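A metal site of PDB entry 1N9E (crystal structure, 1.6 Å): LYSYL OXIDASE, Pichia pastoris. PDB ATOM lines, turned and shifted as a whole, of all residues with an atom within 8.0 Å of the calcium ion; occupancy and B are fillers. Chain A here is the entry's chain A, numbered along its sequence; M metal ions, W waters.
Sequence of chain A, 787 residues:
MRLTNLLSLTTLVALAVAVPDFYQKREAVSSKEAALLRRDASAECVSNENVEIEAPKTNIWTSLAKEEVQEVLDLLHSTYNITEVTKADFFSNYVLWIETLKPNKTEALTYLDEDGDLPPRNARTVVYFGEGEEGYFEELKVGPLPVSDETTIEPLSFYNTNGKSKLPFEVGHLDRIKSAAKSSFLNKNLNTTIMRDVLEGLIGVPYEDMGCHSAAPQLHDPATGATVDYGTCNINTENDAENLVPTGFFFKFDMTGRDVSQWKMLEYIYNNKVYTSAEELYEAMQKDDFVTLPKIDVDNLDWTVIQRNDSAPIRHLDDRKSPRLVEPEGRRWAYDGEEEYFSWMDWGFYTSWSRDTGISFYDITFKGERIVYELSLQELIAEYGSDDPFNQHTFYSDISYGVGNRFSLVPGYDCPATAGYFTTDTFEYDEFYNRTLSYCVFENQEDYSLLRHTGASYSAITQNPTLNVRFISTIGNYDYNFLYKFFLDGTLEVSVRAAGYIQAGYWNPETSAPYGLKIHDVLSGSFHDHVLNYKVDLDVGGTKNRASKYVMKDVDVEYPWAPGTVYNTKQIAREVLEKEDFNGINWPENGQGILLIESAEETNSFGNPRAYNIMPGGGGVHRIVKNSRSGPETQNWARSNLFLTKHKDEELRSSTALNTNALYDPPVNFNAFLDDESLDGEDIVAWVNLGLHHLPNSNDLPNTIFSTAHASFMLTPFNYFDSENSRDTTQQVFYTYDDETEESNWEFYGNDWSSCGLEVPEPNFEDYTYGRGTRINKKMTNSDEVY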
ATOM      1  N   LYS A 105      12.763 -10.571 -34.288  1.00  0.00           N
ATOM      2  CA  LYS A 105      12.986 -10.824 -32.877  1.00  0.00           C
ATOM      3  C   LYS A 105      14.434 -10.839 -32.431  1.00  0.00           C
ATOM      4  O   LYS A 105      14.784 -10.280 -31.386  1.00  0.00           O
ATOM      5  CB  LYS A 105      12.319 -12.142 -32.469  1.00  0.00           C
ATOM      6  CG  LYS A 105      12.431 -12.417 -30.981  1.00  0.00           C
ATOM      7  CD  LYS A 105      11.578 -13.643 -30.613  1.00  0.00           C
ATOM      8  CE  LYS A 105      11.705 -13.937 -29.127  1.00  0.00           C
ATOM      9  NZ  LYS A 105      10.757 -15.050 -28.720  1.00  0.00           N
ATOM     10  N   ILE A 371       9.297 -12.522 -19.401  1.00  0.00           N
ATOM     11  CA  ILE A 371       8.494 -13.751 -19.496  1.00  0.00           C
ATOM     12  C   ILE A 371       7.793 -13.874 -20.864  1.00  0.00           C
ATOM     13  O   ILE A 371       7.533 -14.966 -21.316  1.00  0.00           O
ATOM     14  CB  ILE A 371       7.488 -13.924 -18.352  1.00  0.00           C
ATOM     15  CG1 ILE A 371       6.519 -12.746 -18.293  1.00  0.00           C
ATOM     16  CG2 ILE A 371       8.216 -14.071 -17.014  1.00  0.00           C
ATOM     17  CD1 ILE A 371       5.267 -13.070 -17.448  1.00  0.00           C
ATOM     18  N   VAL A 372       7.501 -12.753 -21.508  1.00  0.00           N
ATOM     19  CA  VAL A 372       6.781 -12.786 -22.793  1.00  0.00           C
ATOM     20  C   VAL A 372       7.410 -11.758 -23.720  1.00  0.00           C
ATOM     21  O   VAL A 372       7.426 -10.566 -23.411  1.00  0.00           O
ATOM     22  CB  VAL A 372       5.283 -12.438 -22.630  1.00  0.00           C
ATOM     23  CG1 VAL A 372       4.619 -12.366 -24.002  1.00  0.00           C
ATOM     24  CG2 VAL A 372       4.576 -13.456 -21.742  1.00  0.00           C
ATOM     25  N   TYR A 373       7.930 -12.216 -24.871  1.00  0.00           N
ATOM     26  CA  TYR A 373       8.507 -11.278 -25.833  1.00  0.00           C
ATOM     27  C   TYR A 373       7.414 -10.455 -26.531  1.00  0.00           C
ATOM     28  O   TYR A 373       7.536  -9.237 -26.678  1.00  0.00           O
ATOM     29  CB  TYR A 373       9.375 -12.005 -26.928  1.00  0.00           C
ATOM     30  CG  TYR A 373       9.737 -10.990 -27.994  1.00  0.00           C
ATOM     31  CD1 TYR A 373      10.700 -10.013 -27.738  1.00  0.00           C
ATOM     32  CD2 TYR A 373       9.101 -10.994 -29.227  1.00  0.00           C
ATOM     33  CE1 TYR A 373      11.032  -9.075 -28.703  1.00  0.00           C
ATOM     34  CE2 TYR A 373       9.431 -10.050 -30.201  1.00  0.00           C
ATOM     35  CZ  TYR A 373      10.395  -9.097 -29.924  1.00  0.00           C
ATOM     36  OH  TYR A 373      10.722  -8.166 -30.894  1.00  0.00           O
ATOM     37  N   GLU A 374       6.340 -11.130 -26.948  1.00  0.00           N
ATOM     38  CA  GLU A 374       5.224 -10.477 -27.629  1.00  0.00           C
ATOM     39  C   GLU A 374       3.906 -11.119 -27.172  1.00  0.00           C
ATOM     40  O   GLU A 374       3.804 -12.348 -27.143  1.00  0.00           O
ATOM     41  CB  GLU A 374       5.376 -10.659 -29.162  1.00  0.00           C
ATOM     42  CG  GLU A 374       4.154 -10.165 -29.934  1.00  0.00           C
ATOM     43  CD  GLU A 374       4.248 -10.394 -31.438  1.00  0.00           C
ATOM     44  OE1 GLU A 374       3.291  -9.983 -32.143  1.00  0.00           O
ATOM     45  OE2 GLU A 374       5.242 -10.972 -31.927  1.00  0.00           O
ATOM     46  N   VAL A 536       0.972 -15.594 -28.186  1.00  0.00           N
ATOM     47  CA  VAL A 536       1.540 -15.518 -26.836  1.00  0.00           C
ATOM     48  C   VAL A 536       2.955 -16.071 -26.932  1.00  0.00           C
ATOM     49  O   VAL A 536       3.184 -17.254 -26.767  1.00  0.00           O
ATOM     50  CB  VAL A 536       0.712 -16.355 -25.825  1.00  0.00           C
ATOM     51  CG1 VAL A 536       1.192 -16.093 -24.392  1.00  0.00           C
ATOM     52  CG2 VAL A 536      -0.796 -16.024 -25.946  1.00  0.00           C
ATOM     53  N   ASP A 537       3.900 -15.183 -27.217  1.00  0.00           N
ATOM     54  CA  ASP A 537       5.276 -15.615 -27.339  1.00  0.00           C
ATOM     55  C   ASP A 537       5.962 -15.604 -25.979  1.00  0.00           C
ATOM     56  O   ASP A 537       6.762 -14.708 -25.673  1.00  0.00           O
ATOM     57  CB  ASP A 537       5.986 -14.728 -28.380  1.00  0.00           C
ATOM     58  CG  ASP A 537       7.395 -15.161 -28.651  1.00  0.00           C
ATOM     59  OD1 ASP A 537       7.798 -16.259 -28.178  1.00  0.00           O
ATOM     60  OD2 ASP A 537       8.164 -14.444 -29.332  1.00  0.00           O
ATOM     61  N   LEU A 538       5.625 -16.602 -25.156  1.00  0.00           N
ATOM     62  CA  LEU A 538       6.292 -16.814 -23.872  1.00  0.00           C
ATOM     63  C   LEU A 538       7.729 -17.203 -24.133  1.00  0.00           C
ATOM     64  O   LEU A 538       8.012 -17.988 -25.051  1.00  0.00           O
ATOM     65  CB  LEU A 538       5.626 -17.984 -23.134  1.00  0.00           C
ATOM     66  CG  LEU A 538       4.359 -17.595 -22.355  1.00  0.00           C
ATOM     67  CD1 LEU A 538       3.337 -18.781 -22.325  1.00  0.00           C
ATOM     68  CD2 LEU A 538       4.741 -17.143 -20.953  1.00  0.00           C
ATOM     69  N   ASP A 539       8.620 -16.658 -23.323  1.00  0.00           N
ATOM     70  CA  ASP A 539      10.038 -17.006 -23.340  1.00  0.00           C
ATOM     71  C   ASP A 539      10.363 -17.221 -21.865  1.00  0.00           C
ATOM     72  O   ASP A 539      10.811 -16.292 -21.191  1.00  0.00           O
ATOM     73  CB  ASP A 539      10.904 -15.829 -23.813  1.00  0.00           C
ATOM     74  CG  ASP A 539      10.911 -15.619 -25.315  1.00  0.00           C
ATOM     75  OD1 ASP A 539      10.402 -16.472 -26.098  1.00  0.00           O
ATOM     76  OD2 ASP A 539      11.439 -14.591 -25.795  1.00  0.00           O
ATOM     77  N   VAL A 540      10.136 -18.432 -21.350  1.00  0.00           N
ATOM     78  CA  VAL A 540      10.279 -18.722 -19.913  1.00  0.00           C
ATOM     79  C   VAL A 540      11.706 -19.117 -19.568  1.00  0.00           C
ATOM     80  O   VAL A 540      12.180 -20.156 -20.001  1.00  0.00           O
ATOM     81  CB  VAL A 540       9.282 -19.847 -19.480  1.00  0.00           C
ATOM     82  CG1 VAL A 540       9.376 -20.103 -17.965  1.00  0.00           C
ATOM     83  CG2 VAL A 540       7.860 -19.458 -19.865  1.00  0.00           C
ATOM     84  N   GLY A 542      14.518 -17.700 -20.621  1.00  0.00           N
ATOM     85  CA  GLY A 542      15.183 -17.658 -21.917  1.00  0.00           C
ATOM     86  C   GLY A 542      14.274 -17.962 -23.097  1.00  0.00           C
ATOM     87  O   GLY A 542      13.118 -18.329 -22.916  1.00  0.00           O
ATOM     88  N   THR A 543      14.771 -17.803 -24.314  1.00  0.00           N
ATOM     89  CA  THR A 543      13.971 -18.168 -25.481  1.00  0.00           C
ATOM     90  C   THR A 543      13.873 -19.668 -25.692  1.00  0.00           C
ATOM     91  O   THR A 543      12.873 -20.173 -26.171  1.00  0.00           O
ATOM     92  CB  THR A 543      14.557 -17.592 -26.776  1.00  0.00           C
ATOM     93  OG1 THR A 543      15.951 -17.946 -26.852  1.00  0.00           O
ATOM     94  CG2 THR A 543      14.587 -16.103 -26.738  1.00  0.00           C
ATOM     95  N   LYS A 544      14.928 -20.412 -25.342  1.00  0.00           N
ATOM     96  CA  LYS A 544      14.918 -21.835 -25.593  1.00  0.00           C
ATOM     97  C   LYS A 544      14.003 -22.551 -24.587  1.00  0.00           C
ATOM     98  O   LYS A 544      14.315 -22.605 -23.403  1.00  0.00           O
ATOM     99  CB  LYS A 544      16.344 -22.402 -25.557  1.00  0.00           C
ATOM    100  CG  LYS A 544      16.431 -23.859 -26.024  1.00  0.00           C
ATOM    101  CD  LYS A 544      17.870 -24.382 -25.988  1.00  0.00           C
ATOM    102  CE  LYS A 544      17.892 -25.881 -26.268  1.00  0.00           C
ATOM    103  NZ  LYS A 544      19.223 -26.367 -26.736  1.00  0.00           N
ATOM    104  N   ASN A 545      12.894 -23.087 -25.067  1.00  0.00           N
ATOM    105  CA  ASN A 545      11.918 -23.670 -24.158  1.00  0.00           C
ATOM    106  C   ASN A 545      11.448 -25.057 -24.602  1.00  0.00           C
ATOM    107  O   ASN A 545      11.856 -25.561 -25.654  1.00  0.00           O
ATOM    108  CB  ASN A 545      10.669 -22.761 -24.121  1.00  0.00           C
ATOM    109  CG  ASN A 545      10.882 -21.409 -23.415  1.00  0.00           C
ATOM    110  OD1 ASN A 545       9.987 -20.563 -23.479  1.00  0.00           O
ATOM    111  ND2 ASN A 545      12.039 -21.193 -22.750  1.00  0.00           N
ATOM    112  N   ILE A 597       4.714 -24.052 -20.451  1.00  0.00           N
ATOM    113  CA  ILE A 597       5.852 -23.699 -21.268  1.00  0.00           C
ATOM    114  C   ILE A 597       7.028 -23.659 -20.288  1.00  0.00           C
ATOM    115  O   ILE A 597       7.044 -22.842 -19.367  1.00  0.00           O
ATOM    116  CB  ILE A 597       5.726 -22.319 -21.949  1.00  0.00           C
ATOM    117  CG1 ILE A 597       4.549 -22.297 -22.927  1.00  0.00           C
ATOM    118  CG2 ILE A 597       7.000 -22.003 -22.731  1.00  0.00           C
ATOM    119  CD1 ILE A 597       4.632 -23.374 -23.991  1.00  0.00           C
ATOM    120  N   THR A 645       3.827 -23.521 -31.879  1.00  0.00           N
ATOM    121  CA  THR A 645       4.737 -23.543 -33.031  1.00  0.00           C
ATOM    122  C   THR A 645       6.125 -23.069 -32.676  1.00  0.00           C
ATOM    123  O   THR A 645       6.365 -22.430 -31.632  1.00  0.00           O
ATOM    124  CB  THR A 645       4.224 -22.710 -34.208  1.00  0.00           C
ATOM    125  OG1 THR A 645       4.217 -21.314 -33.864  1.00  0.00           O
ATOM    126  CG2 THR A 645       2.761 -23.057 -34.543  1.00  0.00           C
ATOM    127  N   LYS A 646       7.055 -23.381 -33.560  1.00  0.00           N
ATOM    128  CA  LYS A 646       8.409 -22.833 -33.451  1.00  0.00           C
ATOM    129  C   LYS A 646       8.396 -21.393 -33.936  1.00  0.00           C
ATOM    130  O   LYS A 646       7.929 -21.099 -35.051  1.00  0.00           O
ATOM    131  CB  LYS A 646       9.377 -23.658 -34.315  1.00  0.00           C
ATOM    132  CG  LYS A 646      10.801 -23.127 -34.360  1.00  0.00           C
ATOM    133  CD  LYS A 646      11.572 -23.997 -35.419  1.00  0.00           C
ATOM    134  CE  LYS A 646      13.017 -23.607 -35.590  1.00  0.00           C
ATOM    135  NZ  LYS A 646      13.654 -24.671 -36.460  1.00  0.00           N
ATOM    136  N   HIS A 647       8.899 -20.478 -33.101  1.00  0.00           N
ATOM    137  CA  HIS A 647       8.948 -19.090 -33.498  1.00  0.00           C
ATOM    138  C   HIS A 647       9.679 -18.811 -34.813  1.00  0.00           C
ATOM    139  O   HIS A 647      10.772 -19.338 -35.050  1.00  0.00           O
ATOM    140  CB  HIS A 647       9.621 -18.220 -32.436  1.00  0.00           C
ATOM    141  CG  HIS A 647       9.699 -16.790 -32.848  1.00  0.00           C
ATOM    142  ND1 HIS A 647      10.766 -16.274 -33.576  1.00  0.00           N
ATOM    143  CD2 HIS A 647       8.855 -15.760 -32.629  1.00  0.00           C
ATOM    144  CE1 HIS A 647      10.548 -14.996 -33.791  1.00  0.00           C
ATOM    145  NE2 HIS A 647       9.406 -14.653 -33.232  1.00  0.00           N
ATOM    146  N   GLU A 682      13.377 -25.220 -28.096  1.00  0.00           N
ATOM    147  CA  GLU A 682      13.255 -24.289 -29.199  1.00  0.00           C
ATOM    148  C   GLU A 682      12.520 -23.047 -28.713  1.00  0.00           C
ATOM    149  O   GLU A 682      11.925 -23.071 -27.633  1.00  0.00           O
ATOM    150  CB  GLU A 682      12.447 -24.900 -30.362  1.00  0.00           C
ATOM    151  CG  GLU A 682      12.945 -26.213 -30.980  1.00  0.00           C
ATOM    152  CD  GLU A 682      14.214 -26.050 -31.796  1.00  0.00           C
ATOM    153  OE1 GLU A 682      14.558 -24.903 -32.182  1.00  0.00           O
ATOM    154  OE2 GLU A 682      14.839 -27.100 -32.049  1.00  0.00           O
ATOM    155  N   ASP A 683      12.567 -21.984 -29.502  1.00  0.00           N
ATOM    156  CA  ASP A 683      11.773 -20.792 -29.192  1.00  0.00           C
ATOM    157  C   ASP A 683      10.334 -21.091 -29.619  1.00  0.00           C
ATOM    158  O   ASP A 683      10.053 -21.261 -30.806  1.00  0.00           O
ATOM    159  CB  ASP A 683      12.294 -19.595 -29.983  1.00  0.00           C
ATOM    160  CG  ASP A 683      11.592 -18.321 -29.613  1.00  0.00           C
ATOM    161  OD1 ASP A 683      10.537 -18.367 -28.917  1.00  0.00           O
ATOM    162  OD2 ASP A 683      12.018 -17.209 -29.988  1.00  0.00           O
ATOM    163  N   ILE A 684       9.439 -21.165 -28.648  1.00  0.00           N
ATOM    164  CA  ILE A 684       8.073 -21.619 -28.899  1.00  0.00           C
ATOM    165  C   ILE A 684       7.143 -20.430 -28.804  1.00  0.00           C
ATOM    166  O   ILE A 684       7.393 -19.502 -28.035  1.00  0.00           O
ATOM    167  CB  ILE A 684       7.647 -22.665 -27.829  1.00  0.00           C
ATOM    168  CG1 ILE A 684       8.476 -23.939 -27.947  1.00  0.00           C
ATOM    169  CG2 ILE A 684       6.143 -23.006 -27.950  1.00  0.00           C
ATOM    170  CD1 ILE A 684       8.264 -24.944 -26.783  1.00  0.00           C
ATOM    171  N   VAL A 685       6.089 -20.480 -29.599  1.00  0.00           N
ATOM    172  CA  VAL A 685       5.004 -19.487 -29.550  1.00  0.00           C
ATOM    173  C   VAL A 685       3.709 -20.275 -29.331  1.00  0.00           C
ATOM    174  O   VAL A 685       3.495 -21.314 -29.973  1.00  0.00           O
ATOM    175  CB  VAL A 685       4.890 -18.706 -30.867  1.00  0.00           C
ATOM    176  CG1 VAL A 685       3.713 -17.713 -30.825  1.00  0.00           C
ATOM    177  CG2 VAL A 685       6.194 -17.949 -31.154  1.00  0.00           C
ATOM    178  N   ALA A 686       2.853 -19.795 -28.415  1.00  0.00           N
ATOM    179  CA  ALA A 686       1.547 -20.401 -28.201  1.00  0.00           C
ATOM    180  C   ALA A 686       0.534 -19.481 -28.853  1.00  0.00           C
ATOM    181  O   ALA A 686       0.554 -18.285 -28.626  1.00  0.00           O
ATOM    182  CB  ALA A 686       1.260 -20.561 -26.713  1.00  0.00           C
HETATM  183 CA    CA M   1       9.003 -17.976 -27.210  1.00  0.00          CA
HETATM  184  O   HOH W   1      10.184 -19.833 -26.073  1.00  0.00           O
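The backbone carbonyl oxygen (O) of Asp 683 sits at hydrogen-bond distance from the backbone NH (N) of His 647 (2.7 Å).
The side-chain amino group (NZ) of Lys 105 is in salt-bridge range of the side-chain carboxylate (OD2) of Asp 683, 2.8 Å away.
The side-chain amino group of Lys 105 lies within salt-bridge range of the side-chain carboxylate of Asp 537 (2.7 Å).
The side-chain amino group (NZ) of Lys 105 lies within salt-bridge range of the side-chain carboxylate (OD2) of Asp 539, at 3.0 Å.
The backbone NH (N) of Asp 539 sits at hydrogen-bond distance from the backbone carbonyl oxygen (O) of Ile 371, at 2.8 Å.
The backbone carbonyl oxygen of Asp 537 sits at hydrogen-bond distance from the backbone NH of Tyr 373 (2.9 Å).
O of Glu 374 sits at hydrogen-bond distance from N of Asp 537, 2.8 Å away.
Residues that only touch the calcium ion: Lys 105 (3.7 Å).
Of the 23 residues printed, 6 come within 4 Å of the calcium ion.
Along chain A the residues within 4 Å of the calcium ion span positions 105 to 684.
The nearest printed residue that does not touch the calcium ion is Val 685 (4.5 Å).
The calcium ion is bound by the side-chain carboxylate of Asp 537 (2.3 Å), the side-chain carboxylate of Asp 683 (2.3 Å), the side-chain carboxylate of Asp 539 (2.3 Å), the backbone carbonyl oxygen of Ile 684 (2.4 Å), the backbone carbonyl oxygen of Leu 538 (2.4 Å) and water W1 (2.5 Å).
The calcium ion has six donor atoms within binding distance.
Water W1 lies within hydrogen-bond range of OD1 of Asn 545 (2.7 Å), O of Thr 543 (2.7 Å) and N of Ile 684 (3.0 Å).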
